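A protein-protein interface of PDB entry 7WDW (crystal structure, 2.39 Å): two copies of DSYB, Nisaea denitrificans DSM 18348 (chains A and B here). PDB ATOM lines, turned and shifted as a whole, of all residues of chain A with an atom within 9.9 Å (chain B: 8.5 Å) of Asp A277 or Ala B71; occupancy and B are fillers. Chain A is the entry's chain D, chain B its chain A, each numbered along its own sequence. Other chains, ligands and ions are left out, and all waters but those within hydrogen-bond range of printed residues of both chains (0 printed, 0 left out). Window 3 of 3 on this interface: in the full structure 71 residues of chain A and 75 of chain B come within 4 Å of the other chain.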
ATOM      1  N   THR A   2      -1.360   3.616 -12.226  1.00  0.00           N
ATOM      2  CA  THR A   2      -0.936   3.863 -10.855  1.00  0.00           C
ATOM      3  C   THR A   2      -2.045   4.517 -10.048  1.00  0.00           C
ATOM      4  O   THR A   2      -2.973   5.105 -10.607  1.00  0.00           O
ATOM      5  CB  THR A   2       0.322   4.769 -10.772  1.00  0.00           C
ATOM      6  OG1 THR A   2      -0.071   6.085 -10.371  1.00  0.00           O
ATOM      7  CG2 THR A   2       1.013   4.872 -12.114  1.00  0.00           C
ATOM      8  N   LEU A   3      -1.911   4.425  -8.728  1.00  0.00           N
ATOM      9  CA  LEU A   3      -2.856   4.969  -7.762  1.00  0.00           C
ATOM     10  C   LEU A   3      -1.978   5.566  -6.650  1.00  0.00           C
ATOM     11  O   LEU A   3      -1.231   4.853  -5.994  1.00  0.00           O
ATOM     12  CB  LEU A   3      -3.725   3.828  -7.239  1.00  0.00           C
ATOM     13  CG  LEU A   3      -5.138   4.033  -6.739  1.00  0.00           C
ATOM     14  CD1 LEU A   3      -5.919   4.772  -7.809  1.00  0.00           C
ATOM     15  CD2 LEU A   3      -5.788   2.686  -6.443  1.00  0.00           C
ATOM     16  N   VAL A 273     -10.730  12.848 -26.669  1.00  0.00           N
ATOM     17  CA  VAL A 273     -11.613  11.756 -26.306  1.00  0.00           C
ATOM     18  C   VAL A 273     -10.952  10.888 -25.267  1.00  0.00           C
ATOM     19  O   VAL A 273      -9.789  10.533 -25.410  1.00  0.00           O
ATOM     20  CB  VAL A 273     -11.956  10.898 -27.545  1.00  0.00           C
ATOM     21  CG1 VAL A 273     -12.982   9.836 -27.190  1.00  0.00           C
ATOM     22  CG2 VAL A 273     -12.481  11.788 -28.658  1.00  0.00           C
ATOM     23  N   VAL A 274     -11.662  10.561 -24.198  1.00  0.00           N
ATOM     24  CA  VAL A 274     -11.103   9.604 -23.254  1.00  0.00           C
ATOM     25  C   VAL A 274     -11.634   8.225 -23.587  1.00  0.00           C
ATOM     26  O   VAL A 274     -12.563   8.083 -24.387  1.00  0.00           O
ATOM     27  CB  VAL A 274     -11.419   9.922 -21.789  1.00  0.00           C
ATOM     28  CG1 VAL A 274     -10.768  11.249 -21.363  1.00  0.00           C
ATOM     29  CG2 VAL A 274     -12.923   9.900 -21.547  1.00  0.00           C
ATOM     30  N   THR A 275     -11.024   7.208 -22.985  1.00  0.00           N
ATOM     31  CA  THR A 275     -11.454   5.841 -23.191  1.00  0.00           C
ATOM     32  C   THR A 275     -12.623   5.557 -22.270  1.00  0.00           C
ATOM     33  O   THR A 275     -12.779   6.198 -21.232  1.00  0.00           O
ATOM     34  CB  THR A 275     -10.320   4.846 -22.906  1.00  0.00           C
ATOM     35  OG1 THR A 275      -9.848   5.034 -21.570  1.00  0.00           O
ATOM     36  CG2 THR A 275      -9.169   5.062 -23.874  1.00  0.00           C
ATOM     37  N   ALA A 276     -13.440   4.589 -22.657  1.00  0.00           N
ATOM     38  CA  ALA A 276     -14.627   4.240 -21.890  1.00  0.00           C
ATOM     39  C   ALA A 276     -14.341   3.878 -20.430  1.00  0.00           C
ATOM     40  O   ALA A 276     -15.207   4.019 -19.581  1.00  0.00           O
ATOM     41  CB  ALA A 276     -15.401   3.122 -22.578  1.00  0.00           C
ATOM     42  N   ASP A 277     -13.141   3.417 -20.123  1.00  0.00           N
ATOM     43  CA  ASP A 277     -12.861   3.022 -18.741  1.00  0.00           C
ATOM     44  C   ASP A 277     -12.489   4.253 -17.917  1.00  0.00           C
ATOM     45  O   ASP A 277     -12.314   4.175 -16.700  1.00  0.00           O
ATOM     46  CB  ASP A 277     -11.793   1.916 -18.659  1.00  0.00           C
ATOM     47  CG  ASP A 277     -10.404   2.414 -18.963  1.00  0.00           C
ATOM     48  OD1 ASP A 277     -10.256   3.578 -19.395  1.00  0.00           O
ATOM     49  OD2 ASP A 277      -9.445   1.633 -18.770  1.00  0.00           O
ATOM     50  N   ARG A 278     -12.384   5.380 -18.620  1.00  0.00           N
ATOM     51  CA  ARG A 278     -12.115   6.695 -18.036  1.00  0.00           C
ATOM     52  C   ARG A 278     -10.835   6.700 -17.208  1.00  0.00           C
ATOM     53  O   ARG A 278     -10.799   7.144 -16.066  1.00  0.00           O
ATOM     54  CB  ARG A 278     -13.353   7.236 -17.306  1.00  0.00           C
ATOM     55  CG  ARG A 278     -14.552   7.223 -18.248  1.00  0.00           C
ATOM     56  CD  ARG A 278     -15.820   7.910 -17.770  1.00  0.00           C
ATOM     57  NE  ARG A 278     -16.663   8.148 -18.940  1.00  0.00           N
ATOM     58  CZ  ARG A 278     -16.571   9.238 -19.698  1.00  0.00           C
ATOM     59  NH1 ARG A 278     -15.700  10.196 -19.359  1.00  0.00           N
ATOM     60  NH2 ARG A 278     -17.349   9.383 -20.779  1.00  0.00           N
ATOM     61  N   THR A 279      -9.780   6.199 -17.840  1.00  0.00           N
ATOM     62  CA  THR A 279      -8.483   6.047 -17.222  1.00  0.00           C
ATOM     63  C   THR A 279      -7.492   6.973 -17.910  1.00  0.00           C
ATOM     64  O   THR A 279      -6.357   7.105 -17.481  1.00  0.00           O
ATOM     65  CB  THR A 279      -7.996   4.600 -17.411  1.00  0.00           C
ATOM     66  OG1 THR A 279      -6.927   4.331 -16.506  1.00  0.00           O
ATOM     67  CG2 THR A 279      -7.522   4.368 -18.860  1.00  0.00           C
ATOM     68  N   GLY A 280      -7.927   7.597 -18.999  1.00  0.00           N
ATOM     69  CA  GLY A 280      -7.061   8.438 -19.806  1.00  0.00           C
ATOM     70  C   GLY A 280      -7.557   8.506 -21.235  1.00  0.00           C
ATOM     71  O   GLY A 280      -8.679   8.087 -21.519  1.00  0.00           O
ATOM     72  N   PRO A 281      -6.734   9.043 -22.145  1.00  0.00           N
ATOM     73  CA  PRO A 281      -5.395   9.551 -21.845  1.00  0.00           C
ATOM     74  C   PRO A 281      -5.449  10.822 -20.989  1.00  0.00           C
ATOM     75  O   PRO A 281      -6.318  11.658 -21.216  1.00  0.00           O
ATOM     76  CB  PRO A 281      -4.813   9.850 -23.237  1.00  0.00           C
ATOM     77  CG  PRO A 281      -5.699   9.134 -24.215  1.00  0.00           C
ATOM     78  CD  PRO A 281      -7.056   9.173 -23.577  1.00  0.00           C
ATOM     79  N   LYS A 282      -4.540  10.933 -20.018  1.00  0.00           N
ATOM     80  CA  LYS A 282      -4.426  12.086 -19.126  1.00  0.00           C
ATOM     81  C   LYS A 282      -4.641  13.445 -19.807  1.00  0.00           C
ATOM     82  O   LYS A 282      -5.393  14.279 -19.304  1.00  0.00           O
ATOM     83  CB  LYS A 282      -3.057  12.090 -18.426  1.00  0.00           C
ATOM     84  CG  LYS A 282      -2.773  13.356 -17.613  1.00  0.00           C
ATOM     85  CD  LYS A 282      -1.360  13.403 -17.039  1.00  0.00           C
ATOM     86  CE  LYS A 282      -0.297  13.747 -18.078  1.00  0.00           C
ATOM     87  NZ  LYS A 282       1.080  13.440 -17.587  1.00  0.00           N
ATOM     88  N   ALA A 285      -8.171  14.012 -21.001  1.00  0.00           N
ATOM     89  CA  ALA A 285      -9.041  14.163 -19.843  1.00  0.00           C
ATOM     90  C   ALA A 285      -8.936  15.575 -19.290  1.00  0.00           C
ATOM     91  O   ALA A 285      -9.927  16.133 -18.848  1.00  0.00           O
ATOM     92  CB  ALA A 285      -8.708  13.139 -18.757  1.00  0.00           C
ATOM     93  N   SER A 300     -18.248  14.674 -21.010  1.00  0.00           N
ATOM     94  CA  SER A 300     -17.084  13.867 -21.418  1.00  0.00           C
ATOM     95  C   SER A 300     -17.354  13.025 -22.675  1.00  0.00           C
ATOM     96  O   SER A 300     -18.225  12.155 -22.669  1.00  0.00           O
ATOM     97  CB  SER A 300     -16.630  12.957 -20.262  1.00  0.00           C
ATOM     98  OG  SER A 300     -15.226  12.734 -20.281  1.00  0.00           O
ATOM     99  N   LEU A 301     -16.623  13.300 -23.753  1.00  0.00           N
ATOM    100  CA  LEU A 301     -16.645  12.441 -24.936  1.00  0.00           C
ATOM    101  C   LEU A 301     -15.781  11.229 -24.665  1.00  0.00           C
ATOM    102  O   LEU A 301     -14.584  11.374 -24.437  1.00  0.00           O
ATOM    103  CB  LEU A 301     -16.012  13.152 -26.123  1.00  0.00           C
ATOM    104  CG  LEU A 301     -16.773  14.108 -27.023  1.00  0.00           C
ATOM    105  CD1 LEU A 301     -15.763  14.856 -27.906  1.00  0.00           C
ATOM    106  CD2 LEU A 301     -17.824  13.379 -27.867  1.00  0.00           C
ATOM    107  N   ASP A 302     -16.356  10.038 -24.685  1.00  0.00           N
ATOM    108  CA  ASP A 302     -15.538   8.841 -24.589  1.00  0.00           C
ATOM    109  C   ASP A 302     -15.685   8.064 -25.889  1.00  0.00           C
ATOM    110  O   ASP A 302     -16.640   8.274 -26.632  1.00  0.00           O
ATOM    111  CB  ASP A 302     -15.915   7.990 -23.369  1.00  0.00           C
ATOM    112  CG  ASP A 302     -17.273   7.328 -23.511  1.00  0.00           C
ATOM    113  OD1 ASP A 302     -17.344   6.252 -24.139  1.00  0.00           O
ATOM    114  OD2 ASP A 302     -18.271   7.870 -22.987  1.00  0.00           O
ATOM    115  N   ASP A 303     -14.728   7.184 -26.168  1.00  0.00           N
ATOM    116  CA  ASP A 303     -14.676   6.464 -27.439  1.00  0.00           C
ATOM    117  C   ASP A 303     -15.848   5.506 -27.681  1.00  0.00           C
ATOM    118  O   ASP A 303     -16.272   5.323 -28.815  1.00  0.00           O
ATOM    119  CB  ASP A 303     -13.345   5.720 -27.592  1.00  0.00           C
ATOM    120  CG  ASP A 303     -13.017   4.822 -26.397  1.00  0.00           C
ATOM    121  OD1 ASP A 303     -13.920   4.494 -25.590  1.00  0.00           O
ATOM    122  OD2 ASP A 303     -11.834   4.433 -26.270  1.00  0.00           O
ATOM    123  N   GLU A 304     -16.367   4.896 -26.626  1.00  0.00           N
ATOM    124  CA  GLU A 304     -17.461   3.938 -26.781  1.00  0.00           C
ATOM    125  C   GLU A 304     -18.767   4.644 -27.118  1.00  0.00           C
ATOM    126  O   GLU A 304     -19.436   4.290 -28.095  1.00  0.00           O
ATOM    127  CB  GLU A 304     -17.613   3.052 -25.533  1.00  0.00           C
ATOM    128  CG  GLU A 304     -17.254   1.584 -25.796  1.00  0.00           C
ATOM    129  CD  GLU A 304     -16.541   0.914 -24.621  1.00  0.00           C
ATOM    130  OE1 GLU A 304     -15.334   0.610 -24.749  1.00  0.00           O
ATOM    131  OE2 GLU A 304     -17.192   0.683 -23.576  1.00  0.00           O
ATOM    132  N   TRP A 305     -19.117   5.644 -26.310  1.00  0.00           N
ATOM    133  CA  TRP A 305     -20.258   6.493 -26.605  1.00  0.00           C
ATOM    134  C   TRP A 305     -20.206   6.962 -28.052  1.00  0.00           C
ATOM    135  O   TRP A 305     -21.189   6.900 -28.753  1.00  0.00           O
ATOM    136  CB  TRP A 305     -20.319   7.722 -25.690  1.00  0.00           C
ATOM    137  CG  TRP A 305     -21.432   8.634 -26.093  1.00  0.00           C
ATOM    138  CD1 TRP A 305     -22.720   8.598 -25.646  1.00  0.00           C
ATOM    139  CD2 TRP A 305     -21.378   9.682 -27.071  1.00  0.00           C
ATOM    140  NE1 TRP A 305     -23.469   9.562 -26.275  1.00  0.00           N
ATOM    141  CE2 TRP A 305     -22.671  10.243 -27.155  1.00  0.00           C
ATOM    142  CE3 TRP A 305     -20.362  10.204 -27.880  1.00  0.00           C
ATOM    143  CZ2 TRP A 305     -22.973  11.307 -28.010  1.00  0.00           C
ATOM    144  CZ3 TRP A 305     -20.667  11.260 -28.737  1.00  0.00           C
ATOM    145  CH2 TRP A 305     -21.962  11.800 -28.793  1.00  0.00           C
ATOM    146  N   LEU B  40     -18.214   5.108  -5.259  1.00  0.00           N
ATOM    147  CA  LEU B  40     -19.465   5.751  -5.645  1.00  0.00           C
ATOM    148  C   LEU B  40     -19.549   5.856  -7.169  1.00  0.00           C
ATOM    149  O   LEU B  40     -18.544   6.092  -7.847  1.00  0.00           O
ATOM    150  CB  LEU B  40     -19.544   7.149  -5.028  1.00  0.00           C
ATOM    151  CG  LEU B  40     -20.528   7.461  -3.901  1.00  0.00           C
ATOM    152  CD1 LEU B  40     -20.794   6.270  -2.989  1.00  0.00           C
ATOM    153  CD2 LEU B  40     -20.016   8.653  -3.116  1.00  0.00           C
ATOM    154  N   LEU B  60     -13.947  13.633 -12.273  1.00  0.00           N
ATOM    155  CA  LEU B  60     -13.400  12.360 -11.812  1.00  0.00           C
ATOM    156  C   LEU B  60     -12.535  11.682 -12.865  1.00  0.00           C
ATOM    157  O   LEU B  60     -11.479  11.136 -12.546  1.00  0.00           O
ATOM    158  CB  LEU B  60     -14.517  11.414 -11.397  1.00  0.00           C
ATOM    159  CG  LEU B  60     -15.174  11.758 -10.069  1.00  0.00           C
ATOM    160  CD1 LEU B  60     -16.442  10.943  -9.932  1.00  0.00           C
ATOM    161  CD2 LEU B  60     -14.205  11.488  -8.910  1.00  0.00           C
ATOM    162  N   THR B  61     -12.980  11.709 -14.119  1.00  0.00           N
ATOM    163  CA  THR B  61     -12.176  11.134 -15.187  1.00  0.00           C
ATOM    164  C   THR B  61     -10.791  11.748 -15.157  1.00  0.00           C
ATOM    165  O   THR B  61      -9.811  11.056 -15.313  1.00  0.00           O
ATOM    166  CB  THR B  61     -12.829  11.331 -16.579  1.00  0.00           C
ATOM    167  OG1 THR B  61     -14.080  10.642 -16.597  1.00  0.00           O
ATOM    168  CG2 THR B  61     -11.941  10.784 -17.711  1.00  0.00           C
ATOM    169  N   ALA B  62     -10.717  13.050 -14.937  1.00  0.00           N
ATOM    170  CA  ALA B  62      -9.446  13.738 -14.955  1.00  0.00           C
ATOM    171  C   ALA B  62      -8.630  13.253 -13.769  1.00  0.00           C
ATOM    172  O   ALA B  62      -7.450  12.923 -13.906  1.00  0.00           O
ATOM    173  CB  ALA B  62      -9.652  15.247 -14.897  1.00  0.00           C
ATOM    174  N   LEU B  63      -9.283  13.207 -12.609  1.00  0.00           N
ATOM    175  CA  LEU B  63      -8.686  12.705 -11.378  1.00  0.00           C
ATOM    176  C   LEU B  63      -8.170  11.278 -11.530  1.00  0.00           C
ATOM    177  O   LEU B  63      -7.065  10.979 -11.120  1.00  0.00           O
ATOM    178  CB  LEU B  63      -9.703  12.762 -10.243  1.00  0.00           C
ATOM    179  CG  LEU B  63     -10.026  14.173  -9.789  1.00  0.00           C
ATOM    180  CD1 LEU B  63     -11.139  14.139  -8.740  1.00  0.00           C
ATOM    181  CD2 LEU B  63      -8.761  14.877  -9.268  1.00  0.00           C
ATOM    182  N   ALA B  64      -8.970  10.401 -12.135  1.00  0.00           N
ATOM    183  CA  ALA B  64      -8.572   9.012 -12.271  1.00  0.00           C
ATOM    184  C   ALA B  64      -7.318   8.916 -13.129  1.00  0.00           C
ATOM    185  O   ALA B  64      -6.428   8.111 -12.858  1.00  0.00           O
ATOM    186  CB  ALA B  64      -9.699   8.178 -12.852  1.00  0.00           C
ATOM    187  N   SER B  65      -7.240   9.760 -14.150  1.00  0.00           N
ATOM    188  CA  SER B  65      -6.109   9.704 -15.068  1.00  0.00           C
ATOM    189  C   SER B  65      -4.815  10.210 -14.410  1.00  0.00           C
ATOM    190  O   SER B  65      -3.718   9.988 -14.914  1.00  0.00           O
ATOM    191  CB  SER B  65      -6.415  10.486 -16.348  1.00  0.00           C
ATOM    192  OG  SER B  65      -6.341  11.880 -16.113  1.00  0.00           O
ATOM    193  N   GLY B  67      -4.259   9.363 -11.260  1.00  0.00           N
ATOM    194  CA  GLY B  67      -4.062   8.414 -10.189  1.00  0.00           C
ATOM    195  C   GLY B  67      -4.596   8.858  -8.844  1.00  0.00           C
ATOM    196  O   GLY B  67      -4.399   8.165  -7.851  1.00  0.00           O
ATOM    197  N   VAL B  68      -5.267  10.002  -8.784  1.00  0.00           N
ATOM    198  CA  VAL B  68      -5.757  10.495  -7.497  1.00  0.00           C
ATOM    199  C   VAL B  68      -6.989   9.699  -7.005  1.00  0.00           C
ATOM    200  O   VAL B  68      -7.285   9.655  -5.808  1.00  0.00           O
ATOM    201  CB  VAL B  68      -6.092  12.012  -7.539  1.00  0.00           C
ATOM    202  CG1 VAL B  68      -6.352  12.537  -6.122  1.00  0.00           C
ATOM    203  CG2 VAL B  68      -4.973  12.805  -8.213  1.00  0.00           C
ATOM    204  N   VAL B  69      -7.704   9.087  -7.940  1.00  0.00           N
ATOM    205  CA  VAL B  69      -8.805   8.202  -7.598  1.00  0.00           C
ATOM    206  C   VAL B  69      -8.762   7.008  -8.527  1.00  0.00           C
ATOM    207  O   VAL B  69      -8.163   7.069  -9.601  1.00  0.00           O
ATOM    208  CB  VAL B  69     -10.192   8.886  -7.772  1.00  0.00           C
ATOM    209  CG1 VAL B  69     -10.334  10.111  -6.849  1.00  0.00           C
ATOM    210  CG2 VAL B  69     -10.447   9.245  -9.251  1.00  0.00           C
ATOM    211  N   SER B  70      -9.416   5.929  -8.115  1.00  0.00           N
ATOM    212  CA  SER B  70      -9.515   4.723  -8.928  1.00  0.00           C
ATOM    213  C   SER B  70     -10.811   4.709  -9.726  1.00  0.00           C
ATOM    214  O   SER B  70     -11.833   5.260  -9.294  1.00  0.00           O
ATOM    215  CB  SER B  70      -9.453   3.473  -8.048  1.00  0.00           C
ATOM    216  OG  SER B  70     -10.501   3.466  -7.094  1.00  0.00           O
ATOM    217  N   ALA B  71     -10.767   4.065 -10.883  1.00  0.00           N
ATOM    218  CA  ALA B  71     -11.930   4.000 -11.754  1.00  0.00           C
ATOM    219  C   ALA B  71     -12.192   2.570 -12.167  1.00  0.00           C
ATOM    220  O   ALA B  71     -11.588   2.078 -13.113  1.00  0.00           O
ATOM    221  CB  ALA B  71     -11.746   4.919 -13.004  1.00  0.00           C
ATOM    222  N   VAL B  72     -13.106   1.914 -11.458  1.00  0.00           N
ATOM    223  CA  VAL B  72     -13.396   0.497 -11.688  1.00  0.00           C
ATOM    224  C   VAL B  72     -14.887   0.204 -11.867  1.00  0.00           C
ATOM    225  O   VAL B  72     -15.663   0.321 -10.921  1.00  0.00           O
ATOM    226  CB  VAL B  72     -12.874  -0.370 -10.516  1.00  0.00           C
ATOM    227  CG1 VAL B  72     -13.270  -1.835 -10.723  1.00  0.00           C
ATOM    228  CG2 VAL B  72     -11.367  -0.199 -10.348  1.00  0.00           C
ATOM    229  N   GLU B  73     -15.269  -0.211 -13.074  1.00  0.00           N
ATOM    230  CA  GLU B  73     -16.668  -0.520 -13.413  1.00  0.00           C
ATOM    231  C   GLU B  73     -17.608   0.632 -13.108  1.00  0.00           C
ATOM    232  O   GLU B  73     -18.591   0.458 -12.390  1.00  0.00           O
ATOM    233  CB  GLU B  73     -17.173  -1.779 -12.692  1.00  0.00           C
ATOM    234  CG  GLU B  73     -16.850  -3.099 -13.384  1.00  0.00           C
ATOM    235  CD  GLU B  73     -17.394  -3.191 -14.810  1.00  0.00           C
ATOM    236  OE1 GLU B  73     -16.586  -3.473 -15.724  1.00  0.00           O
ATOM    237  OE2 GLU B  73     -18.617  -2.998 -15.024  1.00  0.00           O
ATOM    238  N   GLY B  74     -17.303   1.803 -13.656  1.00  0.00           N
ATOM    239  CA  GLY B  74     -18.107   2.992 -13.432  1.00  0.00           C
ATOM    240  C   GLY B  74     -18.233   3.439 -11.986  1.00  0.00           C
ATOM    241  O   GLY B  74     -19.099   4.252 -11.670  1.00  0.00           O
ATOM    242  N   ARG B  75     -17.398   2.922 -11.090  1.00  0.00           N
ATOM    243  CA  ARG B  75     -17.418   3.427  -9.716  1.00  0.00           C
ATOM    244  C   ARG B  75     -16.047   3.928  -9.311  1.00  0.00           C
ATOM    245  O   ARG B  75     -15.047   3.253  -9.507  1.00  0.00           O
ATOM    246  CB  ARG B  75     -17.897   2.367  -8.736  1.00  0.00           C
ATOM    247  CG  ARG B  75     -18.826   1.342  -9.340  1.00  0.00           C
ATOM    248  CD  ARG B  75     -19.627   0.664  -8.259  1.00  0.00           C
ATOM    249  NE  ARG B  75     -20.605   1.589  -7.698  1.00  0.00           N
ATOM    250  CZ  ARG B  75     -20.960   1.614  -6.420  1.00  0.00           C
ATOM    251  NH1 ARG B  75     -20.408   0.765  -5.561  1.00  0.00           N
ATOM    252  NH2 ARG B  75     -21.862   2.489  -5.999  1.00  0.00           N
ATOM    253  N   PHE B  76     -16.009   5.117  -8.738  1.00  0.00           N
ATOM    254  CA  PHE B  76     -14.753   5.751  -8.382  1.00  0.00           C
ATOM    255  C   PHE B  76     -14.513   5.595  -6.899  1.00  0.00           C
ATOM    256  O   PHE B  76     -15.473   5.499  -6.128  1.00  0.00           O
ATOM    257  CB  PHE B  76     -14.776   7.233  -8.766  1.00  0.00           C
ATOM    258  CG  PHE B  76     -14.915   7.465 -10.236  1.00  0.00           C
ATOM    259  CD1 PHE B  76     -16.139   7.282 -10.868  1.00  0.00           C
ATOM    260  CD2 PHE B  76     -13.824   7.854 -10.997  1.00  0.00           C
ATOM    261  CE1 PHE B  76     -16.267   7.483 -12.242  1.00  0.00           C
ATOM    262  CE2 PHE B  76     -13.948   8.062 -12.353  1.00  0.00           C
ATOM    263  CZ  PHE B  76     -15.174   7.878 -12.981  1.00  0.00           C
ATOM    264  N   ALA B  77     -13.232   5.571  -6.515  1.00  0.00           N
ATOM    265  CA  ALA B  77     -12.817   5.475  -5.111  1.00  0.00           C
ATOM    266  C   ALA B  77     -11.513   6.227  -4.874  1.00  0.00           C
ATOM    267  O   ALA B  77     -10.709   6.415  -5.805  1.00  0.00           O
ATOM    268  CB  ALA B  77     -12.665   4.015  -4.689  1.00  0.00           C
ATOM    269  N   ASN B  78     -11.316   6.664  -3.630  1.00  0.00           N
ATOM    270  CA  ASN B  78     -10.077   7.328  -3.223  1.00  0.00           C
ATOM    271  C   ASN B  78      -8.819   6.467  -3.379  1.00  0.00           C
ATOM    272  O   ASN B  78      -8.812   5.283  -3.056  1.00  0.00           O
ATOM    273  CB  ASN B  78     -10.164   7.819  -1.774  1.00  0.00           C
ATOM    274  CG  ASN B  78     -10.960   9.123  -1.636  1.00  0.00           C
ATOM    275  OD1 ASN B  78     -10.955   9.979  -2.531  1.00  0.00           O
ATOM    276  ND2 ASN B  78     -11.643   9.273  -0.507  1.00  0.00           N
ATOM    277  N   SER B  79      -7.756   7.076  -3.888  1.00  0.00           N
ATOM    278  CA  SER B  79      -6.445   6.463  -3.837  1.00  0.00           C
ATOM    279  C   SER B  79      -6.030   6.466  -2.365  1.00  0.00           C
ATOM    280  O   SER B  79      -6.577   7.236  -1.574  1.00  0.00           O
ATOM    281  CB  SER B  79      -5.455   7.276  -4.663  1.00  0.00           C
ATOM    282  OG  SER B  79      -5.224   8.543  -4.073  1.00  0.00           O
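No residue of chain B comes within 4 Å of Ala A276. Of chain B, only Ala B71 comes within 4 Å of Asp A277. Of the printed residues of chain B, Arg A278 touches Thr B61, Ala B64 and Ala B71. Printed residues of chain B within 4 Å of Lys A282: Ser B65. Leu B60 touches none of the printed residues of chain A. Printed residues of chain A within 4 Å of Ser B65: Thr A279, Lys A282 and Ala A285. Of chain A, only Leu A3 comes within 4 Å of Ser B70. Of chain A, only Asp A277 (3.8 Å) and Arg A278 (3.9 Å) come within 4 Å of Ala B71. Val B72 touches none of the printed residues of chain A. The nearest residue of chain A that does not touch Ala B71 is Thr A279 (5.4 Å). The nearest printed residue of chain B that does not touch Leu A3 is Val B68 (5.1 Å).
The side-chain hydroxyl (OG1) of Thr B61 is in hydrogen-bond range of the guanidinium group (NH1) of Arg A278 (3.2 Å).
Printed residues of chain A that touch a printed residue of chain B: Thr A2, Leu A3, Val A274, Asp A277, Arg A278, Thr A279, Lys A282 and Ala A285. Hydrophobic or aromatic side chains of chain A within 4 Å of the printed part of chain B: Leu A3, Val A274 and Ala A285. Of the 20 printed residues of chain B, 9 touch a printed residue of chain A. Printed residues of chain B that touch a printed residue of chain A: Thr B61, Ala B62, Ala B64, Ser B65, Gly B67, Val B69, Ser B70, Ala B71 and Ser B79. Among the printed residues, 14 pairs touch across the chains. Among the printed residues, no Asp or Glu carboxylate lies within 4 Å of a Lys or Arg side-chain nitrogen of the other chain.
No position is printed for both chains.
Gly B67 touches Leu A3. N of Ser B70 touches CD1 of Leu A3, at 3.7 Å. Ser B79 touches Leu A3. Thr B61 touches Val A274. Ala B71 touches Asp A277 (CB to O, 3.8 Å). Arg A278 touches Ala B64. Arg A278 touches Ala B71. Ser B65 touches Lys A282 (OG to CA, 3.6 Å). Ala A285 touches Ala B62 (CB to CA, 3.9 Å). Ser B65 touches Ala A285 (OG to CB, 3.8 Å).
The backbone carbonyl oxygen (O) of Val B68 lies within hydrogen-bond range of the side-chain hydroxyl (OG) of Ser B79 (2.9 Å). The backbone carbonyl oxygen (O) of Ala B77 lies within hydrogen-bond range of the backbone NH (N) of Ser B70 (2.7 Å). N of Val A274 sits at hydrogen-bond distance from O of Leu A301 (3.0 Å). The backbone carbonyl oxygen (O) of Val A274 sits at hydrogen-bond distance from the backbone NH (N) of Asp A303 (2.9 Å). The guanidinium group (NH1) of Arg A278 lies within hydrogen-bond range of the side-chain hydroxyl (OG) of Ser A300 (2.7 Å). The side-chain carboxylate of Asp A302 lies within salt-bridge range of the guanidinium group of Arg A278, at 2.8 Å.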
